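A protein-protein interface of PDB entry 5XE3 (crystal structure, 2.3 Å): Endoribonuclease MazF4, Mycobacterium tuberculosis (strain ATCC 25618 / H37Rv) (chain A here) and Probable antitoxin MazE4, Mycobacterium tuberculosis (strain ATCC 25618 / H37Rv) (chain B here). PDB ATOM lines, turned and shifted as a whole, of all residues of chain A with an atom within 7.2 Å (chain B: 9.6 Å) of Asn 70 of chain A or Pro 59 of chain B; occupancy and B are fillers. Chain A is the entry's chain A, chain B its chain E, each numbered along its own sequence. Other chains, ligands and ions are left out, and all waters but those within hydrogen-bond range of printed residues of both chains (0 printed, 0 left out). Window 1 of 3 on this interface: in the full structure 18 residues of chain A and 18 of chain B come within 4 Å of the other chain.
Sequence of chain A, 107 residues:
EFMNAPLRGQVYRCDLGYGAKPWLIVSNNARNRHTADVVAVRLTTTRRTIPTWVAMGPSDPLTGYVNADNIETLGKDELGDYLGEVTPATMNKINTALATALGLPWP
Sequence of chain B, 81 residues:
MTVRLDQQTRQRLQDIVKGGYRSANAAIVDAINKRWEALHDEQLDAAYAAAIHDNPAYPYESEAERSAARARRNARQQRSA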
ATOM      1  N   LEU A  16      11.789 -14.692 -38.961  1.00  0.00           N
ATOM      2  CA  LEU A  16      12.071 -13.256 -38.891  1.00  0.00           C
ATOM      3  C   LEU A  16      13.532 -12.896 -38.985  1.00  0.00           C
ATOM      4  O   LEU A  16      13.846 -11.728 -38.925  1.00  0.00           O
ATOM      5  CB  LEU A  16      11.490 -12.642 -37.612  1.00  0.00           C
ATOM      6  CG  LEU A  16      10.096 -12.053 -37.774  1.00  0.00           C
ATOM      7  CD1 LEU A  16       9.105 -13.064 -38.349  1.00  0.00           C
ATOM      8  CD2 LEU A  16       9.668 -11.514 -36.408  1.00  0.00           C
ATOM      9  N   TYR A  18      15.920 -15.276 -37.385  1.00  0.00           N
ATOM     10  CA  TYR A  18      16.545 -16.135 -36.376  1.00  0.00           C
ATOM     11  C   TYR A  18      15.919 -17.540 -36.348  1.00  0.00           C
ATOM     12  O   TYR A  18      15.853 -18.182 -35.294  1.00  0.00           O
ATOM     13  CB  TYR A  18      16.429 -15.472 -35.000  1.00  0.00           C
ATOM     14  CG  TYR A  18      15.068 -14.839 -34.661  1.00  0.00           C
ATOM     15  CD1 TYR A  18      14.070 -15.561 -33.997  1.00  0.00           C
ATOM     16  CD2 TYR A  18      14.797 -13.492 -34.967  1.00  0.00           C
ATOM     17  CE1 TYR A  18      12.842 -14.970 -33.654  1.00  0.00           C
ATOM     18  CE2 TYR A  18      13.575 -12.901 -34.643  1.00  0.00           C
ATOM     19  CZ  TYR A  18      12.605 -13.641 -33.989  1.00  0.00           C
ATOM     20  OH  TYR A  18      11.419 -13.059 -33.662  1.00  0.00           O
ATOM     21  N   TRP A  23       3.646 -18.224 -35.260  1.00  0.00           N
ATOM     22  CA  TRP A  23       3.113 -16.879 -35.008  1.00  0.00           C
ATOM     23  C   TRP A  23       1.613 -16.930 -35.109  1.00  0.00           C
ATOM     24  O   TRP A  23       1.081 -17.418 -36.093  1.00  0.00           O
ATOM     25  CB  TRP A  23       3.662 -15.861 -36.034  1.00  0.00           C
ATOM     26  CG  TRP A  23       5.171 -15.651 -35.897  1.00  0.00           C
ATOM     27  CD1 TRP A  23       6.151 -16.395 -36.474  1.00  0.00           C
ATOM     28  CD2 TRP A  23       5.847 -14.678 -35.071  1.00  0.00           C
ATOM     29  NE1 TRP A  23       7.404 -15.957 -36.055  1.00  0.00           N
ATOM     30  CE2 TRP A  23       7.235 -14.907 -35.201  1.00  0.00           C
ATOM     31  CE3 TRP A  23       5.408 -13.631 -34.243  1.00  0.00           C
ATOM     32  CZ2 TRP A  23       8.176 -14.140 -34.542  1.00  0.00           C
ATOM     33  CZ3 TRP A  23       6.350 -12.877 -33.560  1.00  0.00           C
ATOM     34  CH2 TRP A  23       7.728 -13.127 -33.724  1.00  0.00           C
ATOM     35  N   ALA A  40       0.936 -10.248 -35.534  1.00  0.00           N
ATOM     36  CA  ALA A  40       0.909 -11.524 -34.912  1.00  0.00           C
ATOM     37  C   ALA A  40       1.703 -11.554 -33.593  1.00  0.00           C
ATOM     38  O   ALA A  40       2.539 -10.718 -33.388  1.00  0.00           O
ATOM     39  CB  ALA A  40       1.491 -12.522 -35.881  1.00  0.00           C
ATOM     40  N   VAL A  41       1.448 -12.562 -32.744  1.00  0.00           N
ATOM     41  CA  VAL A  41       2.221 -12.787 -31.513  1.00  0.00           C
ATOM     42  C   VAL A  41       2.968 -14.130 -31.549  1.00  0.00           C
ATOM     43  O   VAL A  41       2.491 -15.116 -32.127  1.00  0.00           O
ATOM     44  CB  VAL A  41       1.369 -12.702 -30.227  1.00  0.00           C
ATOM     45  CG1 VAL A  41       0.874 -11.274 -30.015  1.00  0.00           C
ATOM     46  CG2 VAL A  41       0.177 -13.660 -30.266  1.00  0.00           C
ATOM     47  N   ARG A  42       4.137 -14.136 -30.914  1.00  0.00           N
ATOM     48  CA  ARG A  42       5.019 -15.269 -30.879  1.00  0.00           C
ATOM     49  C   ARG A  42       4.437 -16.440 -30.049  1.00  0.00           C
ATOM     50  O   ARG A  42       4.068 -16.282 -28.875  1.00  0.00           O
ATOM     51  CB  ARG A  42       6.361 -14.789 -30.309  1.00  0.00           C
ATOM     52  CG  ARG A  42       7.456 -15.825 -30.082  1.00  0.00           C
ATOM     53  CD  ARG A  42       7.906 -16.536 -31.347  1.00  0.00           C
ATOM     54  NE  ARG A  42       8.828 -17.601 -30.957  1.00  0.00           N
ATOM     55  CZ  ARG A  42      10.093 -17.418 -30.584  1.00  0.00           C
ATOM     56  NH1 ARG A  42      10.642 -16.210 -30.582  1.00  0.00           N
ATOM     57  NH2 ARG A  42      10.829 -18.461 -30.225  1.00  0.00           N
ATOM     58  N   LEU A  43       4.327 -17.599 -30.696  1.00  0.00           N
ATOM     59  CA  LEU A  43       4.182 -18.879 -30.009  1.00  0.00           C
ATOM     60  C   LEU A  43       5.558 -19.368 -29.624  1.00  0.00           C
ATOM     61  O   LEU A  43       6.520 -19.201 -30.367  1.00  0.00           O
ATOM     62  CB  LEU A  43       3.519 -19.937 -30.879  1.00  0.00           C
ATOM     63  CG  LEU A  43       1.998 -20.073 -30.756  1.00  0.00           C
ATOM     64  CD1 LEU A  43       1.309 -18.733 -30.983  1.00  0.00           C
ATOM     65  CD2 LEU A  43       1.437 -21.111 -31.727  1.00  0.00           C
ATOM     66  N   ARG A  48       6.596 -19.384 -18.983  1.00  0.00           N
ATOM     67  CA  ARG A  48       6.664 -18.239 -18.085  1.00  0.00           C
ATOM     68  C   ARG A  48       5.296 -17.938 -17.456  1.00  0.00           C
ATOM     69  O   ARG A  48       4.249 -18.152 -18.082  1.00  0.00           O
ATOM     70  CB  ARG A  48       7.224 -17.032 -18.835  1.00  0.00           C
ATOM     71  CG  ARG A  48       8.334 -16.323 -18.092  1.00  0.00           C
ATOM     72  CD  ARG A  48       9.153 -15.436 -19.009  1.00  0.00           C
ATOM     73  NE  ARG A  48      10.578 -15.632 -18.760  1.00  0.00           N
ATOM     74  CZ  ARG A  48      11.548 -15.572 -19.675  1.00  0.00           C
ATOM     75  NH1 ARG A  48      11.299 -15.302 -20.970  1.00  0.00           N
ATOM     76  NH2 ARG A  48      12.803 -15.780 -19.282  1.00  0.00           N
ATOM     77  N   THR A  52       0.615 -11.719 -19.393  1.00  0.00           N
ATOM     78  CA  THR A  52       0.717 -11.607 -20.857  1.00  0.00           C
ATOM     79  C   THR A  52       1.029 -12.900 -21.622  1.00  0.00           C
ATOM     80  O   THR A  52       1.060 -12.902 -22.856  1.00  0.00           O
ATOM     81  CB  THR A  52       1.737 -10.561 -21.244  1.00  0.00           C
ATOM     82  OG1 THR A  52       2.934 -10.756 -20.486  1.00  0.00           O
ATOM     83  CG2 THR A  52       1.203  -9.169 -20.942  1.00  0.00           C
ATOM     84  N   TRP A  53       1.202 -14.010 -20.904  1.00  0.00           N
ATOM     85  CA  TRP A  53       1.361 -15.297 -21.542  1.00  0.00           C
ATOM     86  C   TRP A  53       0.170 -16.221 -21.328  1.00  0.00           C
ATOM     87  O   TRP A  53      -0.419 -16.256 -20.245  1.00  0.00           O
ATOM     88  CB  TRP A  53       2.636 -15.943 -21.033  1.00  0.00           C
ATOM     89  CG  TRP A  53       3.924 -15.279 -21.494  1.00  0.00           C
ATOM     90  CD1 TRP A  53       4.199 -13.944 -21.598  1.00  0.00           C
ATOM     91  CD2 TRP A  53       5.121 -15.959 -21.903  1.00  0.00           C
ATOM     92  NE1 TRP A  53       5.476 -13.754 -22.055  1.00  0.00           N
ATOM     93  CE2 TRP A  53       6.066 -14.976 -22.245  1.00  0.00           C
ATOM     94  CE3 TRP A  53       5.479 -17.312 -22.022  1.00  0.00           C
ATOM     95  CZ2 TRP A  53       7.339 -15.301 -22.687  1.00  0.00           C
ATOM     96  CZ3 TRP A  53       6.737 -17.629 -22.469  1.00  0.00           C
ATOM     97  CH2 TRP A  53       7.663 -16.633 -22.780  1.00  0.00           C
ATOM     98  N   ASN A  67       3.117 -15.494 -26.147  1.00  0.00           N
ATOM     99  CA  ASN A  67       3.643 -14.292 -25.493  1.00  0.00           C
ATOM    100  C   ASN A  67       3.110 -13.007 -26.183  1.00  0.00           C
ATOM    101  O   ASN A  67       3.512 -12.700 -27.277  1.00  0.00           O
ATOM    102  CB  ASN A  67       5.148 -14.349 -25.578  1.00  0.00           C
ATOM    103  CG  ASN A  67       5.803 -13.069 -25.173  1.00  0.00           C
ATOM    104  OD1 ASN A  67       5.143 -12.107 -24.796  1.00  0.00           O
ATOM    105  ND2 ASN A  67       7.115 -13.047 -25.250  1.00  0.00           N
ATOM    106  N   ALA A  68       2.215 -12.267 -25.528  1.00  0.00           N
ATOM    107  CA  ALA A  68       1.552 -11.088 -26.127  1.00  0.00           C
ATOM    108  C   ALA A  68       2.312  -9.805 -25.925  1.00  0.00           C
ATOM    109  O   ALA A  68       1.880  -8.766 -26.420  1.00  0.00           O
ATOM    110  CB  ALA A  68       0.135 -10.932 -25.595  1.00  0.00           C
ATOM    111  N   ASP A  69       3.425  -9.830 -25.187  1.00  0.00           N
ATOM    112  CA  ASP A  69       4.346  -8.703 -25.213  1.00  0.00           C
ATOM    113  C   ASP A  69       5.179  -8.622 -26.482  1.00  0.00           C
ATOM    114  O   ASP A  69       5.822  -7.643 -26.722  1.00  0.00           O
ATOM    115  CB  ASP A  69       5.284  -8.761 -24.030  1.00  0.00           C
ATOM    116  CG  ASP A  69       4.587  -8.496 -22.721  1.00  0.00           C
ATOM    117  OD1 ASP A  69       4.141  -7.329 -22.498  1.00  0.00           O
ATOM    118  OD2 ASP A  69       4.521  -9.453 -21.897  1.00  0.00           O
ATOM    119  N   ASN A  70       5.215  -9.669 -27.283  1.00  0.00           N
ATOM    120  CA  ASN A  70       6.068  -9.709 -28.459  1.00  0.00           C
ATOM    121  C   ASN A  70       5.141  -9.723 -29.651  1.00  0.00           C
ATOM    122  O   ASN A  70       4.825 -10.758 -30.241  1.00  0.00           O
ATOM    123  CB  ASN A  70       6.974 -10.942 -28.420  1.00  0.00           C
ATOM    124  CG  ASN A  70       7.953 -11.014 -29.587  1.00  0.00           C
ATOM    125  OD1 ASN A  70       8.152 -10.056 -30.343  1.00  0.00           O
ATOM    126  ND2 ASN A  70       8.564 -12.183 -29.747  1.00  0.00           N
ATOM    127  N   ILE A  71       4.693  -8.537 -29.978  1.00  0.00           N
ATOM    128  CA  ILE A  71       3.874  -8.310 -31.164  1.00  0.00           C
ATOM    129  C   ILE A  71       4.784  -8.004 -32.376  1.00  0.00           C
ATOM    130  O   ILE A  71       5.761  -7.325 -32.253  1.00  0.00           O
ATOM    131  CB  ILE A  71       2.894  -7.158 -30.858  1.00  0.00           C
ATOM    132  CG1 ILE A  71       1.901  -7.609 -29.785  1.00  0.00           C
ATOM    133  CG2 ILE A  71       2.136  -6.718 -32.082  1.00  0.00           C
ATOM    134  CD1 ILE A  71       1.286  -6.448 -29.042  1.00  0.00           C
ATOM    135  N   GLU A  72       4.440  -8.506 -33.556  1.00  0.00           N
ATOM    136  CA  GLU A  72       5.285  -8.318 -34.739  1.00  0.00           C
ATOM    137  C   GLU A  72       4.426  -8.178 -35.950  1.00  0.00           C
ATOM    138  O   GLU A  72       3.368  -8.761 -35.977  1.00  0.00           O
ATOM    139  CB  GLU A  72       6.216  -9.542 -34.953  1.00  0.00           C
ATOM    140  CG  GLU A  72       7.489  -9.502 -34.139  1.00  0.00           C
ATOM    141  CD  GLU A  72       8.433  -8.349 -34.522  1.00  0.00           C
ATOM    142  OE1 GLU A  72       8.151  -7.581 -35.479  1.00  0.00           O
ATOM    143  OE2 GLU A  72       9.474  -8.228 -33.850  1.00  0.00           O
ATOM    144  N   ALA A 101      -1.218  -6.307 -22.279  1.00  0.00           N
ATOM    145  CA  ALA A 101       0.023  -5.835 -22.892  1.00  0.00           C
ATOM    146  C   ALA A 101      -0.051  -4.397 -23.420  1.00  0.00           C
ATOM    147  O   ALA A 101       0.903  -3.650 -23.308  1.00  0.00           O
ATOM    148  CB  ALA A 101       0.460  -6.765 -24.011  1.00  0.00           C
ATOM    149  N   TYR B  48       7.091  -8.624 -14.560  1.00  0.00           N
ATOM    150  CA  TYR B  48       7.999  -8.043 -15.575  1.00  0.00           C
ATOM    151  C   TYR B  48       9.410  -7.945 -15.012  1.00  0.00           C
ATOM    152  O   TYR B  48      10.387  -8.148 -15.744  1.00  0.00           O
ATOM    153  CB  TYR B  48       7.555  -6.657 -16.094  1.00  0.00           C
ATOM    154  CG  TYR B  48       6.510  -6.652 -17.196  1.00  0.00           C
ATOM    155  CD1 TYR B  48       6.821  -7.040 -18.500  1.00  0.00           C
ATOM    156  CD2 TYR B  48       5.200  -6.213 -16.939  1.00  0.00           C
ATOM    157  CE1 TYR B  48       5.850  -7.020 -19.508  1.00  0.00           C
ATOM    158  CE2 TYR B  48       4.245  -6.182 -17.926  1.00  0.00           C
ATOM    159  CZ  TYR B  48       4.561  -6.570 -19.215  1.00  0.00           C
ATOM    160  OH  TYR B  48       3.569  -6.528 -20.165  1.00  0.00           O
ATOM    161  N   ALA B  51      10.818 -11.684 -15.066  1.00  0.00           N
ATOM    162  CA  ALA B  51      11.208 -11.962 -16.485  1.00  0.00           C
ATOM    163  C   ALA B  51      12.468 -11.220 -16.932  1.00  0.00           C
ATOM    164  O   ALA B  51      13.292 -11.797 -17.610  1.00  0.00           O
ATOM    165  CB  ALA B  51      10.087 -11.656 -17.452  1.00  0.00           C
ATOM    166  N   ILE B  52      12.614  -9.957 -16.533  1.00  0.00           N
ATOM    167  CA  ILE B  52      13.789  -9.144 -16.898  1.00  0.00           C
ATOM    168  C   ILE B  52      15.072  -9.551 -16.142  1.00  0.00           C
ATOM    169  O   ILE B  52      16.179  -9.460 -16.684  1.00  0.00           O
ATOM    170  CB  ILE B  52      13.496  -7.642 -16.689  1.00  0.00           C
ATOM    171  CG1 ILE B  52      12.677  -7.117 -17.866  1.00  0.00           C
ATOM    172  CG2 ILE B  52      14.768  -6.782 -16.532  1.00  0.00           C
ATOM    173  CD1 ILE B  52      13.440  -6.915 -19.163  1.00  0.00           C
ATOM    174  N   ASN B  55      15.805 -12.728 -17.978  1.00  0.00           N
ATOM    175  CA  ASN B  55      16.070 -12.475 -19.393  1.00  0.00           C
ATOM    176  C   ASN B  55      16.061 -10.978 -19.657  1.00  0.00           C
ATOM    177  O   ASN B  55      14.992 -10.412 -19.898  1.00  0.00           O
ATOM    178  CB  ASN B  55      15.023 -13.161 -20.279  1.00  0.00           C
ATOM    179  CG  ASN B  55      15.130 -12.749 -21.754  1.00  0.00           C
ATOM    180  OD1 ASN B  55      16.110 -12.120 -22.157  1.00  0.00           O
ATOM    181  ND2 ASN B  55      14.131 -13.108 -22.560  1.00  0.00           N
ATOM    182  N   PRO B  56      17.248 -10.334 -19.664  1.00  0.00           N
ATOM    183  CA  PRO B  56      17.288  -8.891 -19.842  1.00  0.00           C
ATOM    184  C   PRO B  56      16.765  -8.340 -21.172  1.00  0.00           C
ATOM    185  O   PRO B  56      16.612  -7.149 -21.271  1.00  0.00           O
ATOM    186  CB  PRO B  56      18.783  -8.561 -19.688  1.00  0.00           C
ATOM    187  CG  PRO B  56      19.351  -9.690 -18.915  1.00  0.00           C
ATOM    188  CD  PRO B  56      18.610 -10.868 -19.471  1.00  0.00           C
ATOM    189  N   ALA B  57      16.490  -9.188 -22.157  1.00  0.00           N
ATOM    190  CA  ALA B  57      15.922  -8.761 -23.431  1.00  0.00           C
ATOM    191  C   ALA B  57      14.419  -9.035 -23.569  1.00  0.00           C
ATOM    192  O   ALA B  57      13.876  -8.918 -24.695  1.00  0.00           O
ATOM    193  CB  ALA B  57      16.669  -9.448 -24.578  1.00  0.00           C
ATOM    194  N   TYR B  58      13.741  -9.413 -22.480  1.00  0.00           N
ATOM    195  CA  TYR B  58      12.310  -9.684 -22.550  1.00  0.00           C
ATOM    196  C   TYR B  58      11.653  -8.450 -23.180  1.00  0.00           C
ATOM    197  O   TYR B  58      12.012  -7.286 -22.843  1.00  0.00           O
ATOM    198  CB  TYR B  58      11.717  -9.959 -21.171  1.00  0.00           C
ATOM    199  CG  TYR B  58      10.244 -10.319 -21.205  1.00  0.00           C
ATOM    200  CD1 TYR B  58       9.848 -11.636 -21.385  1.00  0.00           C
ATOM    201  CD2 TYR B  58       9.251  -9.333 -21.088  1.00  0.00           C
ATOM    202  CE1 TYR B  58       8.516 -11.970 -21.455  1.00  0.00           C
ATOM    203  CE2 TYR B  58       7.906  -9.661 -21.146  1.00  0.00           C
ATOM    204  CZ  TYR B  58       7.538 -10.963 -21.332  1.00  0.00           C
ATOM    205  OH  TYR B  58       6.211 -11.310 -21.415  1.00  0.00           O
ATOM    206  N   PRO B  59      10.713  -8.678 -24.102  1.00  0.00           N
ATOM    207  CA  PRO B  59      10.036  -9.915 -24.470  1.00  0.00           C
ATOM    208  C   PRO B  59      10.646 -10.721 -25.599  1.00  0.00           C
ATOM    209  O   PRO B  59      10.016 -11.688 -26.073  1.00  0.00           O
ATOM    210  CB  PRO B  59       8.670  -9.401 -24.886  1.00  0.00           C
ATOM    211  CG  PRO B  59       9.011  -8.132 -25.613  1.00  0.00           C
ATOM    212  CD  PRO B  59      10.195  -7.545 -24.905  1.00  0.00           C
ATOM    213  N   TYR B  60      11.830 -10.307 -26.028  1.00  0.00           N
ATOM    214  CA  TYR B  60      12.622 -11.012 -27.016  1.00  0.00           C
ATOM    215  C   TYR B  60      13.458 -12.088 -26.278  1.00  0.00           C
ATOM    216  O   TYR B  60      14.001 -11.837 -25.186  1.00  0.00           O
ATOM    217  CB  TYR B  60      13.572 -10.019 -27.736  1.00  0.00           C
ATOM    218  CG  TYR B  60      12.860  -8.863 -28.447  1.00  0.00           C
ATOM    219  CD1 TYR B  60      12.086  -9.088 -29.578  1.00  0.00           C
ATOM    220  CD2 TYR B  60      12.949  -7.573 -27.982  1.00  0.00           C
ATOM    221  CE1 TYR B  60      11.427  -8.054 -30.210  1.00  0.00           C
ATOM    222  CE2 TYR B  60      12.320  -6.536 -28.630  1.00  0.00           C
ATOM    223  CZ  TYR B  60      11.560  -6.782 -29.745  1.00  0.00           C
ATOM    224  OH  TYR B  60      10.918  -5.748 -30.375  1.00  0.00           O
ATOM    225  N   GLU B  61      13.600 -13.257 -26.890  1.00  0.00           N
ATOM    226  CA  GLU B  61      14.340 -14.367 -26.279  1.00  0.00           C
ATOM    227  C   GLU B  61      15.858 -14.154 -26.261  1.00  0.00           C
ATOM    228  O   GLU B  61      16.513 -14.718 -25.414  1.00  0.00           O
ATOM    229  CB  GLU B  61      13.962 -15.719 -26.920  1.00  0.00           C
ATOM    230  CG  GLU B  61      12.446 -15.960 -26.963  1.00  0.00           C
ATOM    231  CD  GLU B  61      12.005 -17.421 -26.923  1.00  0.00           C
ATOM    232  OE1 GLU B  61      12.786 -18.324 -27.302  1.00  0.00           O
ATOM    233  OE2 GLU B  61      10.840 -17.666 -26.519  1.00  0.00           O
ATOM    234  N   SER B  62      16.395 -13.337 -27.175  1.00  0.00           N
ATOM    235  CA  SER B  62      17.836 -12.968 -27.212  1.00  0.00           C
ATOM    236  C   SER B  62      18.025 -11.561 -27.776  1.00  0.00           C
ATOM    237  O   SER B  62      17.116 -11.026 -28.423  1.00  0.00           O
ATOM    238  CB  SER B  62      18.618 -13.936 -28.112  1.00  0.00           C
ATOM    239  OG  SER B  62      18.234 -13.782 -29.480  1.00  0.00           O
ATOM    240  N   GLU B  63      19.210 -10.980 -27.581  1.00  0.00           N
ATOM    241  CA  GLU B  63      19.541  -9.691 -28.205  1.00  0.00           C
ATOM    242  C   GLU B  63      19.496  -9.723 -29.741  1.00  0.00           C
ATOM    243  O   GLU B  63      19.238  -8.691 -30.366  1.00  0.00           O
ATOM    244  CB  GLU B  63      20.903  -9.167 -27.735  1.00  0.00           C
ATOM    245  CG  GLU B  63      20.947  -8.716 -26.274  1.00  0.00           C
ATOM    246  CD  GLU B  63      20.128  -7.451 -25.956  1.00  0.00           C
ATOM    247  OE1 GLU B  63      19.839  -6.624 -26.862  1.00  0.00           O
ATOM    248  OE2 GLU B  63      19.768  -7.284 -24.762  1.00  0.00           O
ATOM    249  N   GLU B  65      17.252 -11.557 -31.561  1.00  0.00           N
ATOM    250  CA  GLU B  65      15.826 -11.343 -31.848  1.00  0.00           C
ATOM    251  C   GLU B  65      15.423  -9.851 -31.906  1.00  0.00           C
ATOM    252  O   GLU B  65      14.683  -9.439 -32.817  1.00  0.00           O
ATOM    253  CB  GLU B  65      14.927 -12.068 -30.829  1.00  0.00           C
ATOM    254  CG  GLU B  65      14.849 -13.594 -30.970  1.00  0.00           C
ATOM    255  CD  GLU B  65      13.563 -14.217 -30.382  1.00  0.00           C
ATOM    256  OE1 GLU B  65      13.486 -15.470 -30.344  1.00  0.00           O
ATOM    257  OE2 GLU B  65      12.620 -13.485 -29.952  1.00  0.00           O
ATOM    258  N   ARG B  66      15.916  -9.069 -30.952  1.00  0.00           N
ATOM    259  CA  ARG B  66      15.630  -7.622 -30.885  1.00  0.00           C
ATOM    260  C   ARG B  66      16.167  -6.898 -32.132  1.00  0.00           C
ATOM    261  O   ARG B  66      15.492  -6.062 -32.717  1.00  0.00           O
ATOM    262  CB  ARG B  66      16.206  -7.033 -29.599  1.00  0.00           C
ATOM    263  CG  ARG B  66      16.482  -5.541 -29.620  1.00  0.00           C
ATOM    264  CD  ARG B  66      16.860  -5.031 -28.243  1.00  0.00           C
ATOM    265  NE  ARG B  66      15.668  -5.019 -27.410  1.00  0.00           N
ATOM    266  CZ  ARG B  66      15.600  -5.318 -26.111  1.00  0.00           C
ATOM    267  NH1 ARG B  66      16.685  -5.676 -25.410  1.00  0.00           N
ATOM    268  NH2 ARG B  66      14.406  -5.252 -25.508  1.00  0.00           N
ATOM    269  N   ALA B  68      16.963  -8.159 -35.216  1.00  0.00           N
ATOM    270  CA  ALA B  68      16.117  -8.504 -36.325  1.00  0.00           C
ATOM    271  C   ALA B  68      14.839  -7.634 -36.336  1.00  0.00           C
ATOM    272  O   ALA B  68      14.551  -6.999 -37.339  1.00  0.00           O
ATOM    273  CB  ALA B  68      15.770  -9.965 -36.264  1.00  0.00           C
ATOM    274  N   ALA B  69      14.145  -7.552 -35.190  1.00  0.00           N
ATOM    275  CA  ALA B  69      12.886  -6.792 -35.064  1.00  0.00           C
ATOM    276  C   ALA B  69      13.098  -5.298 -35.368  1.00  0.00           C
ATOM    277  O   ALA B  69      12.306  -4.698 -36.118  1.00  0.00           O
ATOM    278  CB  ALA B  69      12.294  -6.982 -33.674  1.00  0.00           C
ATOM    279  N   ARG B  70      14.200  -4.742 -34.863  1.00  0.00           N
ATOM    280  CA  ARG B  70      14.597  -3.349 -35.163  1.00  0.00           C
ATOM    281  C   ARG B  70      14.854  -3.106 -36.644  1.00  0.00           C
ATOM    282  O   ARG B  70      14.356  -2.121 -37.209  1.00  0.00           O
ATOM    283  CB  ARG B  70      15.871  -2.943 -34.428  1.00  0.00           C
ATOM    284  CG  ARG B  70      15.732  -2.895 -32.930  1.00  0.00           C
ATOM    285  CD  ARG B  70      14.961  -1.685 -32.461  1.00  0.00           C
ATOM    286  NE  ARG B  70      14.779  -1.756 -31.013  1.00  0.00           N
ATOM    287  CZ  ARG B  70      13.915  -2.566 -30.385  1.00  0.00           C
ATOM    288  NH1 ARG B  70      13.097  -3.433 -31.041  1.00  0.00           N
ATOM    289  NH2 ARG B  70      13.878  -2.523 -29.073  1.00  0.00           N
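The guanidinium group (NH2) of Arg 42 of chain A lies within salt-bridge range of the side-chain carboxylate (OE1) of Glu 61 of chain B (3.5 Å).
NH1 of Arg 42 of chain A lies within salt-bridge range of OE1 of Glu 65 of chain B, at 2.9 Å.
The side-chain hydroxyl of Thr 52 of chain A lies within hydrogen-bond range of the side-chain hydroxyl of Tyr 58 of chain B, 3.5 Å away.
The side-chain hydroxyl (OH) of Tyr 58 of chain B lies within hydrogen-bond range of the indole nitrogen (NE1) of Trp 53 of chain A, 2.6 Å away.
The side-chain amide nitrogen of Asn 67 of chain A lies within hydrogen-bond range of the backbone carbonyl oxygen of Pro 59 of chain B (3.3 Å).
The side-chain carboxylate of Asp 69 of chain A sits at hydrogen-bond distance from the side-chain hydroxyl of Tyr 48 of chain B (2.5 Å).
The side-chain carboxylate (OD2) of Asp 69 of chain A sits at hydrogen-bond distance from the side-chain hydroxyl (OH) of Tyr 58 of chain B (2.6 Å).
Among the printed residues, pairs that only touch across the chains: Leu 16 of chain A with Ala 68 of chain B (3.7 Å), Tyr 18 of chain A with Glu 65 of chain B (3.4 Å), Tyr 18 of chain A with Ala 68 of chain B (3.9 Å), Arg 48 of chain A with Asn 55 of chain B (3.6 Å), Arg 48 of chain A with Tyr 58 of chain B (3.96 Å), Thr 52 of chain A with Tyr 48 of chain B (3.6 Å), Asn 67 of chain A with Tyr 58 of chain B (3.6 Å), Asp 69 of chain A with Pro 59 of chain B (3.4 Å), Asn 70 of chain A with Pro 59 of chain B (3.9 Å), Asn 70 of chain A with Tyr 60 of chain B (3.8 Å) and Glu 72 of chain A with Ala 69 of chain B (3.1 Å).
O of Glu 72 of chain A lies within hydrogen-bond range of N of Ala 40 of chain A (2.9 Å).
The backbone carbonyl oxygen (O) of Arg 42 of chain A is in hydrogen-bond range of the backbone NH (N) of Asn 67 of chain A, 3.0 Å away.
The backbone NH (N) of Asn 70 of chain A sits at hydrogen-bond distance from the side-chain amide oxygen (OD1) of Asn 67 of chain A, at 3.5 Å.
OD1 of Asn 55 of chain B is in hydrogen-bond range of N of Ala 57 of chain B.
The side-chain hydroxyl of Ser 62 of chain B sits at hydrogen-bond distance from the backbone NH of Glu 65 of chain B (3.2 Å).
Printed residues of chain B that touch a printed residue of chain A: Tyr 48, Asn 55, Tyr 58, Pro 59, Tyr 60, Glu 61, Glu 65, Ala 68 and Ala 69.
Of the 17 printed residues of chain A, 10 touch a printed residue of chain B.
Printed residues of chain A that touch a printed residue of chain B: Leu 16, Tyr 18, Arg 42, Arg 48, Thr 52, Trp 53, Asn 67, Asp 69, Asn 70 and Glu 72.
Hydrophobic or aromatic side chains of chain A within 4 Å of the printed part of chain B: Tyr 18 and Trp 53.
Along chain A the printed residues that touch a printed residue of chain B span positions 16 to 72.
Among the printed residues, Asp or Glu carboxylates within 4 Å of a Lys or Arg side-chain nitrogen of the other chain: Arg 42 of chain A with Glu 61 of chain B and Arg 42 of chain A with Glu 65 of chain B.
Of the printed residues of chain B, Asn 70 of chain A touches Pro 59 and Tyr 60.
Pro 59 of chain B touches just these residues of chain A: Asn 67 (3.3 Å), Asp 69 (3.4 Å) and Asn 70 (3.9 Å).
No residue of chain B comes within 4 Å of Val 41 of chain A.
No residue of chain B comes within 4 Å of Ala 68 of chain A.
No residue of chain B comes within 4 Å of Ile 71 of chain A.
Of the printed residues of chain A, Ala 68 of chain B touches Leu 16 and Tyr 18.
Printed residues of chain A within 4 Å of Tyr 58 of chain B: Arg 48, Thr 52, Trp 53, Asn 67 and Asp 69.
Ser 62 of chain B touches none of the printed residues of chain A.
Ala 101 of chain A touches none of the printed residues of chain B.
The nearest residue of chain B that does not touch Asn 70 of chain A is Glu 65 of chain B (4.3 Å).
The nearest residue of chain A that does not touch Pro 59 of chain B is Trp 53 of chain A (5.6 Å).
The nearest printed residue of chain B that does not touch Tyr 18 of chain A is Ala 69 of chain B (5.4 Å).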
